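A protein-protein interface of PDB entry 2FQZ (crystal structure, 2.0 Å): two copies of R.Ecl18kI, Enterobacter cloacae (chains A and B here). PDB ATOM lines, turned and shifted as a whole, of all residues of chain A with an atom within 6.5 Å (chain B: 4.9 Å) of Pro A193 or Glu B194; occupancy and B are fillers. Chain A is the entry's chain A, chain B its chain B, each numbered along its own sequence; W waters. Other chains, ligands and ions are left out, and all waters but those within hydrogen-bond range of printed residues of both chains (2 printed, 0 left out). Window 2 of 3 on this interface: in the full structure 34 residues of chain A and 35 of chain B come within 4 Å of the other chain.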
ATOM      1  N   GLU A 187     -32.796  28.420   1.256  1.00  0.00           N
ATOM      2  CA  GLU A 187     -32.398  27.493   2.321  1.00  0.00           C
ATOM      3  C   GLU A 187     -31.387  28.123   3.276  1.00  0.00           C
ATOM      4  O   GLU A 187     -30.998  27.498   4.265  1.00  0.00           O
ATOM      5  CB  GLU A 187     -31.787  26.221   1.714  1.00  0.00           C
ATOM      6  CG  GLU A 187     -30.268  26.290   1.439  1.00  0.00           C
ATOM      7  CD  GLU A 187     -29.808  27.358   0.415  1.00  0.00           C
ATOM      8  OE1 GLU A 187     -30.624  28.023  -0.265  1.00  0.00           O
ATOM      9  OE2 GLU A 187     -28.587  27.532   0.284  1.00  0.00           O
ATOM     10  N   ARG A 188     -30.950  29.345   2.958  1.00  0.00           N
ATOM     11  CA  ARG A 188     -29.882  30.041   3.682  1.00  0.00           C
ATOM     12  C   ARG A 188     -30.241  30.410   5.113  1.00  0.00           C
ATOM     13  O   ARG A 188     -29.359  30.672   5.924  1.00  0.00           O
ATOM     14  CB  ARG A 188     -29.434  31.289   2.920  1.00  0.00           C
ATOM     15  CG  ARG A 188     -28.567  30.976   1.685  1.00  0.00           C
ATOM     16  CD  ARG A 188     -28.305  32.254   0.883  1.00  0.00           C
ATOM     17  NE  ARG A 188     -29.488  32.691   0.134  1.00  0.00           N
ATOM     18  CZ  ARG A 188     -30.353  33.612   0.533  1.00  0.00           C
ATOM     19  NH1 ARG A 188     -30.181  34.251   1.681  1.00  0.00           N
ATOM     20  NH2 ARG A 188     -31.400  33.900  -0.235  1.00  0.00           N
ATOM     21  N   TRP A 189     -31.537  30.416   5.414  1.00  0.00           N
ATOM     22  CA  TRP A 189     -32.010  30.509   6.789  1.00  0.00           C
ATOM     23  C   TRP A 189     -31.351  29.487   7.702  1.00  0.00           C
ATOM     24  O   TRP A 189     -31.241  29.722   8.905  1.00  0.00           O
ATOM     25  CB  TRP A 189     -33.527  30.350   6.844  1.00  0.00           C
ATOM     26  CG  TRP A 189     -34.042  29.043   6.380  1.00  0.00           C
ATOM     27  CD1 TRP A 189     -34.549  28.767   5.152  1.00  0.00           C
ATOM     28  CD2 TRP A 189     -34.109  27.822   7.124  1.00  0.00           C
ATOM     29  NE1 TRP A 189     -34.940  27.457   5.081  1.00  0.00           N
ATOM     30  CE2 TRP A 189     -34.673  26.850   6.276  1.00  0.00           C
ATOM     31  CE3 TRP A 189     -33.722  27.447   8.420  1.00  0.00           C
ATOM     32  CZ2 TRP A 189     -34.881  25.531   6.682  1.00  0.00           C
ATOM     33  CZ3 TRP A 189     -33.935  26.157   8.821  1.00  0.00           C
ATOM     34  CH2 TRP A 189     -34.511  25.208   7.966  1.00  0.00           C
ATOM     35  N   GLN A 190     -30.927  28.357   7.127  1.00  0.00           N
ATOM     36  CA  GLN A 190     -30.253  27.303   7.869  1.00  0.00           C
ATOM     37  C   GLN A 190     -28.984  27.767   8.573  1.00  0.00           C
ATOM     38  O   GLN A 190     -28.568  27.173   9.556  1.00  0.00           O
ATOM     39  CB  GLN A 190     -29.981  26.086   6.986  1.00  0.00           C
ATOM     40  CG  GLN A 190     -31.275  25.389   6.568  1.00  0.00           C
ATOM     41  CD  GLN A 190     -31.120  24.453   5.379  1.00  0.00           C
ATOM     42  OE1 GLN A 190     -32.093  23.851   4.943  1.00  0.00           O
ATOM     43  NE2 GLN A 190     -29.922  24.363   4.831  1.00  0.00           N
ATOM     44  N   GLU A 191     -28.405  28.858   8.095  1.00  0.00           N
ATOM     45  CA  GLU A 191     -27.172  29.410   8.680  1.00  0.00           C
ATOM     46  C   GLU A 191     -27.439  29.967  10.062  1.00  0.00           C
ATOM     47  O   GLU A 191     -26.549  30.011  10.910  1.00  0.00           O
ATOM     48  CB  GLU A 191     -26.630  30.527   7.759  1.00  0.00           C
ATOM     49  CG  GLU A 191     -26.167  29.959   6.417  1.00  0.00           C
ATOM     50  CD  GLU A 191     -25.915  31.047   5.379  1.00  0.00           C
ATOM     51  OE1 GLU A 191     -26.053  32.240   5.739  1.00  0.00           O
ATOM     52  OE2 GLU A 191     -25.581  30.692   4.209  1.00  0.00           O
ATOM     53  N   VAL A 192     -28.679  30.380  10.287  1.00  0.00           N
ATOM     54  CA  VAL A 192     -29.017  31.112  11.490  1.00  0.00           C
ATOM     55  C   VAL A 192     -29.099  30.213  12.742  1.00  0.00           C
ATOM     56  O   VAL A 192     -28.453  30.527  13.729  1.00  0.00           O
ATOM     57  CB  VAL A 192     -30.254  32.015  11.312  1.00  0.00           C
ATOM     58  CG1 VAL A 192     -30.403  32.907  12.512  1.00  0.00           C
ATOM     59  CG2 VAL A 192     -30.142  32.876  10.009  1.00  0.00           C
ATOM     60  N   PRO A 193     -29.853  29.091  12.700  1.00  0.00           N
ATOM     61  CA  PRO A 193     -29.756  28.187  13.855  1.00  0.00           C
ATOM     62  C   PRO A 193     -28.323  27.729  14.106  1.00  0.00           C
ATOM     63  O   PRO A 193     -27.916  27.576  15.264  1.00  0.00           O
ATOM     64  CB  PRO A 193     -30.613  26.994  13.441  1.00  0.00           C
ATOM     65  CG  PRO A 193     -31.627  27.583  12.466  1.00  0.00           C
ATOM     66  CD  PRO A 193     -30.806  28.576  11.698  1.00  0.00           C
ATOM     67  N   GLU A 194     -27.553  27.537  13.039  1.00  0.00           N
ATOM     68  CA  GLU A 194     -26.161  27.135  13.197  1.00  0.00           C
ATOM     69  C   GLU A 194     -25.466  28.169  14.060  1.00  0.00           C
ATOM     70  O   GLU A 194     -24.783  27.819  15.027  1.00  0.00           O
ATOM     71  CB  GLU A 194     -25.446  27.028  11.853  1.00  0.00           C
ATOM     72  CG  GLU A 194     -24.020  26.431  11.975  1.00  0.00           C
ATOM     73  CD  GLU A 194     -22.995  27.481  12.297  1.00  0.00           C
ATOM     74  OE1 GLU A 194     -23.218  28.653  11.922  1.00  0.00           O
ATOM     75  OE2 GLU A 194     -21.967  27.138  12.904  1.00  0.00           O
ATOM     76  N   GLU A 195     -25.638  29.445  13.710  1.00  0.00           N
ATOM     77  CA  GLU A 195     -24.966  30.499  14.453  1.00  0.00           C
ATOM     78  C   GLU A 195     -25.514  30.641  15.870  1.00  0.00           C
ATOM     79  O   GLU A 195     -24.763  30.879  16.796  1.00  0.00           O
ATOM     80  CB  GLU A 195     -25.023  31.834  13.683  1.00  0.00           C
ATOM     81  CG  GLU A 195     -23.959  31.847  12.545  1.00  0.00           C
ATOM     82  CD  GLU A 195     -22.553  31.648  13.077  1.00  0.00           C
ATOM     83  OE1 GLU A 195     -22.111  32.548  13.815  1.00  0.00           O
ATOM     84  OE2 GLU A 195     -21.891  30.600  12.802  1.00  0.00           O
ATOM     85  N   VAL A 196     -26.818  30.488  16.032  1.00  0.00           N
ATOM     86  CA  VAL A 196     -27.434  30.565  17.358  1.00  0.00           C
ATOM     87  C   VAL A 196     -26.893  29.448  18.241  1.00  0.00           C
ATOM     88  O   VAL A 196     -26.444  29.650  19.377  1.00  0.00           O
ATOM     89  CB  VAL A 196     -28.978  30.462  17.229  1.00  0.00           C
ATOM     90  CG1 VAL A 196     -29.640  30.170  18.583  1.00  0.00           C
ATOM     91  CG2 VAL A 196     -29.517  31.762  16.551  1.00  0.00           C
ATOM     92  N   ASN A 197     -26.932  28.248  17.714  1.00  0.00           N
ATOM     93  CA  ASN A 197     -26.444  27.138  18.485  1.00  0.00           C
ATOM     94  C   ASN A 197     -24.970  27.123  18.766  1.00  0.00           C
ATOM     95  O   ASN A 197     -24.536  26.630  19.811  1.00  0.00           O
ATOM     96  CB  ASN A 197     -26.934  25.858  17.856  1.00  0.00           C
ATOM     97  CG  ASN A 197     -28.433  25.765  17.933  1.00  0.00           C
ATOM     98  OD1 ASN A 197     -29.025  26.134  18.959  1.00  0.00           O
ATOM     99  ND2 ASN A 197     -29.073  25.319  16.849  1.00  0.00           N
ATOM    100  N   ARG A 198     -24.192  27.654  17.837  1.00  0.00           N
ATOM    101  CA  ARG A 198     -22.760  27.639  17.998  1.00  0.00           C
ATOM    102  C   ARG A 198     -22.303  28.499  19.178  1.00  0.00           C
ATOM    103  O   ARG A 198     -21.374  28.129  19.891  1.00  0.00           O
ATOM    104  CB  ARG A 198     -22.079  28.107  16.713  1.00  0.00           C
ATOM    105  CG  ARG A 198     -20.601  27.864  16.745  1.00  0.00           C
ATOM    106  CD  ARG A 198     -19.921  28.334  15.468  1.00  0.00           C
ATOM    107  NE  ARG A 198     -20.193  29.737  15.160  1.00  0.00           N
ATOM    108  CZ  ARG A 198     -19.525  30.778  15.676  1.00  0.00           C
ATOM    109  NH1 ARG A 198     -18.548  30.586  16.565  1.00  0.00           N
ATOM    110  NH2 ARG A 198     -19.857  32.027  15.323  1.00  0.00           N
ATOM    111  N   ILE A 220     -39.058  25.024  11.948  1.00  0.00           N
ATOM    112  CA  ILE A 220     -37.657  24.719  12.235  1.00  0.00           C
ATOM    113  C   ILE A 220     -36.919  25.892  12.875  1.00  0.00           C
ATOM    114  O   ILE A 220     -36.238  25.717  13.902  1.00  0.00           O
ATOM    115  CB  ILE A 220     -36.929  24.224  10.987  1.00  0.00           C
ATOM    116  CG1 ILE A 220     -37.581  22.912  10.546  1.00  0.00           C
ATOM    117  CG2 ILE A 220     -35.414  24.080  11.276  1.00  0.00           C
ATOM    118  CD1 ILE A 220     -37.240  22.524   9.083  1.00  0.00           C
ATOM    119  N   LEU A 221     -37.046  27.072  12.268  1.00  0.00           N
ATOM    120  CA  LEU A 221     -36.516  28.307  12.863  1.00  0.00           C
ATOM    121  C   LEU A 221     -36.995  28.523  14.285  1.00  0.00           C
ATOM    122  O   LEU A 221     -36.210  28.834  15.199  1.00  0.00           O
ATOM    123  CB  LEU A 221     -36.871  29.518  11.999  1.00  0.00           C
ATOM    124  CG  LEU A 221     -36.041  29.564  10.707  1.00  0.00           C
ATOM    125  CD1 LEU A 221     -36.565  30.674   9.822  1.00  0.00           C
ATOM    126  CD2 LEU A 221     -34.547  29.757  10.982  1.00  0.00           C
ATOM    127  N   ALA A 224     -35.452  26.503  16.822  1.00  0.00           N
ATOM    128  CA  ALA A 224     -34.058  26.923  16.931  1.00  0.00           C
ATOM    129  C   ALA A 224     -33.927  28.278  17.591  1.00  0.00           C
ATOM    130  O   ALA A 224     -32.825  28.787  17.772  1.00  0.00           O
ATOM    131  CB  ALA A 224     -33.418  26.937  15.576  1.00  0.00           C
ATOM    132  N   VAL A 226     -35.030  31.125  16.493  1.00  0.00           N
ATOM    133  CA  VAL A 226     -34.825  32.182  15.519  1.00  0.00           C
ATOM    134  C   VAL A 226     -36.220  32.707  15.223  1.00  0.00           C
ATOM    135  O   VAL A 226     -37.111  31.960  14.788  1.00  0.00           O
ATOM    136  CB  VAL A 226     -34.085  31.687  14.269  1.00  0.00           C
ATOM    137  CG1 VAL A 226     -34.025  32.772  13.185  1.00  0.00           C
ATOM    138  CG2 VAL A 226     -32.652  31.205  14.655  1.00  0.00           C
ATOM    139  N   GLN B 190     -22.314  26.560   6.860  1.00  0.00           N
ATOM    140  CA  GLN B 190     -23.109  26.705   8.093  1.00  0.00           C
ATOM    141  C   GLN B 190     -24.440  25.954   8.030  1.00  0.00           C
ATOM    142  O   GLN B 190     -25.027  25.590   9.066  1.00  0.00           O
ATOM    143  CB  GLN B 190     -23.341  28.189   8.409  1.00  0.00           C
ATOM    144  CG  GLN B 190     -22.080  28.931   8.860  1.00  0.00           C
ATOM    145  CD  GLN B 190     -22.218  30.446   8.746  1.00  0.00           C
ATOM    146  OE1 GLN B 190     -23.254  30.947   8.327  1.00  0.00           O
ATOM    147  NE2 GLN B 190     -21.141  31.166   9.030  1.00  0.00           N
ATOM    148  N   GLU B 191     -24.932  25.718   6.819  1.00  0.00           N
ATOM    149  CA  GLU B 191     -26.164  24.936   6.656  1.00  0.00           C
ATOM    150  C   GLU B 191     -26.020  23.511   7.143  1.00  0.00           C
ATOM    151  O   GLU B 191     -27.005  22.873   7.521  1.00  0.00           O
ATOM    152  CB  GLU B 191     -26.587  24.890   5.189  1.00  0.00           C
ATOM    153  CG  GLU B 191     -26.970  26.264   4.644  1.00  0.00           C
ATOM    154  CD  GLU B 191     -27.097  26.292   3.141  1.00  0.00           C
ATOM    155  OE1 GLU B 191     -26.981  25.209   2.496  1.00  0.00           O
ATOM    156  OE2 GLU B 191     -27.288  27.418   2.614  1.00  0.00           O
ATOM    157  N   VAL B 192     -24.799  22.997   7.085  1.00  0.00           N
ATOM    158  CA  VAL B 192     -24.600  21.580   7.340  1.00  0.00           C
ATOM    159  C   VAL B 192     -24.703  21.270   8.819  1.00  0.00           C
ATOM    160  O   VAL B 192     -25.441  20.358   9.182  1.00  0.00           O
ATOM    161  CB  VAL B 192     -23.289  21.037   6.732  1.00  0.00           C
ATOM    162  CG1 VAL B 192     -23.269  19.542   6.887  1.00  0.00           C
ATOM    163  CG2 VAL B 192     -23.232  21.410   5.254  1.00  0.00           C
ATOM    164  N   PRO B 193     -23.994  22.023   9.678  1.00  0.00           N
ATOM    165  CA  PRO B 193     -24.256  21.752  11.096  1.00  0.00           C
ATOM    166  C   PRO B 193     -25.708  21.941  11.497  1.00  0.00           C
ATOM    167  O   PRO B 193     -26.229  21.201  12.350  1.00  0.00           O
ATOM    168  CB  PRO B 193     -23.357  22.754  11.831  1.00  0.00           C
ATOM    169  CG  PRO B 193     -22.316  23.118  10.890  1.00  0.00           C
ATOM    170  CD  PRO B 193     -22.942  23.041   9.511  1.00  0.00           C
ATOM    171  N   GLU B 194     -26.370  22.930  10.918  1.00  0.00           N
ATOM    172  CA  GLU B 194     -27.783  23.072  11.172  1.00  0.00           C
ATOM    173  C   GLU B 194     -28.542  21.764  10.919  1.00  0.00           C
ATOM    174  O   GLU B 194     -29.322  21.316  11.763  1.00  0.00           O
ATOM    175  CB  GLU B 194     -28.367  24.200  10.325  1.00  0.00           C
ATOM    176  CG  GLU B 194     -29.813  24.536  10.723  1.00  0.00           C
ATOM    177  CD  GLU B 194     -30.850  23.654  10.073  1.00  0.00           C
ATOM    178  OE1 GLU B 194     -30.612  23.111   8.975  1.00  0.00           O
ATOM    179  OE2 GLU B 194     -31.950  23.543  10.652  1.00  0.00           O
ATOM    180  N   GLU B 195     -28.330  21.166   9.752  1.00  0.00           N
ATOM    181  CA  GLU B 195     -29.041  19.936   9.412  1.00  0.00           C
ATOM    182  C   GLU B 195     -28.601  18.757  10.280  1.00  0.00           C
ATOM    183  O   GLU B 195     -29.420  17.933  10.689  1.00  0.00           O
ATOM    184  CB  GLU B 195     -28.879  19.649   7.914  1.00  0.00           C
ATOM    185  CG  GLU B 195     -29.695  20.666   7.095  1.00  0.00           C
ATOM    186  CD  GLU B 195     -31.179  20.477   7.329  1.00  0.00           C
ATOM    187  OE1 GLU B 195     -31.660  19.418   6.884  1.00  0.00           O
ATOM    188  OE2 GLU B 195     -31.849  21.330   7.990  1.00  0.00           O
ATOM    189  N   VAL B 196     -27.313  18.671  10.564  1.00  0.00           N
ATOM    190  CA  VAL B 196     -26.807  17.609  11.436  1.00  0.00           C
ATOM    191  C   VAL B 196     -27.484  17.757  12.789  1.00  0.00           C
ATOM    192  O   VAL B 196     -28.086  16.825  13.317  1.00  0.00           O
ATOM    193  CB  VAL B 196     -25.255  17.648  11.522  1.00  0.00           C
ATOM    194  CG1 VAL B 196     -24.735  16.840  12.722  1.00  0.00           C
ATOM    195  CG2 VAL B 196     -24.643  17.124  10.185  1.00  0.00           C
ATOM    196  N   ASN B 197     -27.451  18.961  13.329  1.00  0.00           N
ATOM    197  CA  ASN B 197     -28.012  19.161  14.649  1.00  0.00           C
ATOM    198  C   ASN B 197     -29.537  19.009  14.689  1.00  0.00           C
ATOM    199  O   ASN B 197     -30.076  18.466  15.646  1.00  0.00           O
ATOM    200  CB  ASN B 197     -27.503  20.472  15.246  1.00  0.00           C
ATOM    201  CG  ASN B 197     -26.046  20.364  15.668  1.00  0.00           C
ATOM    202  OD1 ASN B 197     -25.295  21.352  15.665  1.00  0.00           O
ATOM    203  ND2 ASN B 197     -25.635  19.147  16.056  1.00  0.00           N
ATOM    204  N   ARG B 198     -30.210  19.416  13.615  1.00  0.00           N
ATOM    205  CA  ARG B 198     -31.657  19.280  13.529  1.00  0.00           C
ATOM    206  C   ARG B 198     -32.142  17.834  13.594  1.00  0.00           C
ATOM    207  O   ARG B 198     -33.148  17.548  14.237  1.00  0.00           O
ATOM    208  CB  ARG B 198     -32.187  19.950  12.265  1.00  0.00           C
ATOM    209  CG  ARG B 198     -33.687  20.179  12.272  1.00  0.00           C
ATOM    210  CD  ARG B 198     -34.104  20.905  10.998  1.00  0.00           C
ATOM    211  NE  ARG B 198     -33.793  20.149   9.785  1.00  0.00           N
ATOM    212  CZ  ARG B 198     -34.523  19.136   9.318  1.00  0.00           C
ATOM    213  NH1 ARG B 198     -35.606  18.732   9.967  1.00  0.00           N
ATOM    214  NH2 ARG B 198     -34.156  18.516   8.211  1.00  0.00           N
HETATM  215  O   HOH W   1     -27.511  25.212  -0.776  1.00  0.00           O
HETATM  216  O   HOH W   2     -27.086  24.058  14.714  1.00  0.00           O
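Of the 9 printed residues of chain B, 6 touch a printed residue of chain A. Printed residues of chain B that touch a printed residue of chain A: Gln B190, Glu B191, Pro B193, Glu B194, Glu B195 and Arg B198. Hydrophobic or aromatic side chains of chain B within 4 Å of the printed part of chain A: Pro B193. Hydrophobic or aromatic side chains of chain A within 4 Å of the printed part of chain B: Trp A189, Pro A193 and Ile A220. Among the printed residues, no Asp or Glu carboxylate lies within 4 Å of a Lys or Arg side-chain nitrogen of the other chain.
NE2 of Gln A190 lies close to O of Glu A187, 3.4 Å away. OE2 of Glu A194 lies within salt-bridge range of NE of Arg A198, 3.9 Å away. OE1 of Glu A194 lies close to OE2 of Glu A195 (2.5 Å). The backbone carbonyl oxygen (O) of Pro A193 sits at hydrogen-bond distance from the side-chain amide nitrogen (ND2) of Asn A197 (3.0 Å). The side-chain carboxylate (OE2) of Glu B194 is in salt-bridge range of the guanidinium group (NE) of Arg B198 (3.96 Å). O of Pro B193 sits close to OD1 of Asn B197 (3.4 Å).
Water W1 bridges OE2 of Glu A187 (2.8 Å) and OE1 of Glu B191 (3.3 Å). Water W2 lies within hydrogen-bond range of ND2 of Asn A197 and OD1 of Asn B197.
The side-chain carboxylate (OE2) of Glu A187 sits close to the side-chain carboxylate (OE2) of Glu B191 (2.7 Å).
Among the printed residues, pairs that only touch across the chains: Arg A188 with Glu B191, Trp A189 with Glu B194, Gln A190 with Gln B190, Gln A190 with Glu B191, Gln A190 with Glu B194, Gln A190 with Glu B195, Glu A191 with Gln B190, Pro A193 with Glu B194, Glu A194 with Gln B190, Glu A194 with Pro B193, Glu A195 with Gln B190, Ile A220 with Glu B194 and Ile A220 with Arg B198.
Gln A190 touches Glu B191, and with the chains exchanged Glu A191 touches Gln B190. Gln A190 touches Glu B194, and with the chains exchanged Glu A194 touches Gln B190. Gln A190 touches Glu B195, and with the chains exchanged Glu A195 touches Gln B190. Pro A193 touches Glu B194, and with the chains exchanged Glu A194 touches Pro B193.
Of the printed residues of chain B, Pro A193 touches Glu B194. Glu B194 touches four residues of chain A. Of the printed residues of chain B, Arg A188 touches Glu B191 (3.8 Å). Of the printed residues of chain A, Glu B195 touches Gln A190 (3.96 Å). Printed residues of chain B within 4 Å of Trp A189: Glu B194. Printed residues of chain A within 4 Å of Pro B193: Glu A194. Printed residues of chain B within 4 Å of Glu A195: Gln B190 (3.9 Å). Val A192 touches none of the printed residues of chain B. Val A226 touches none of the printed residues of chain B. The nearest printed residue of chain B that does not touch Pro A193 is Gln B190 (6.4 Å). The nearest residue of chain A that does not touch Glu B194 is Glu A194 (4.3 Å).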
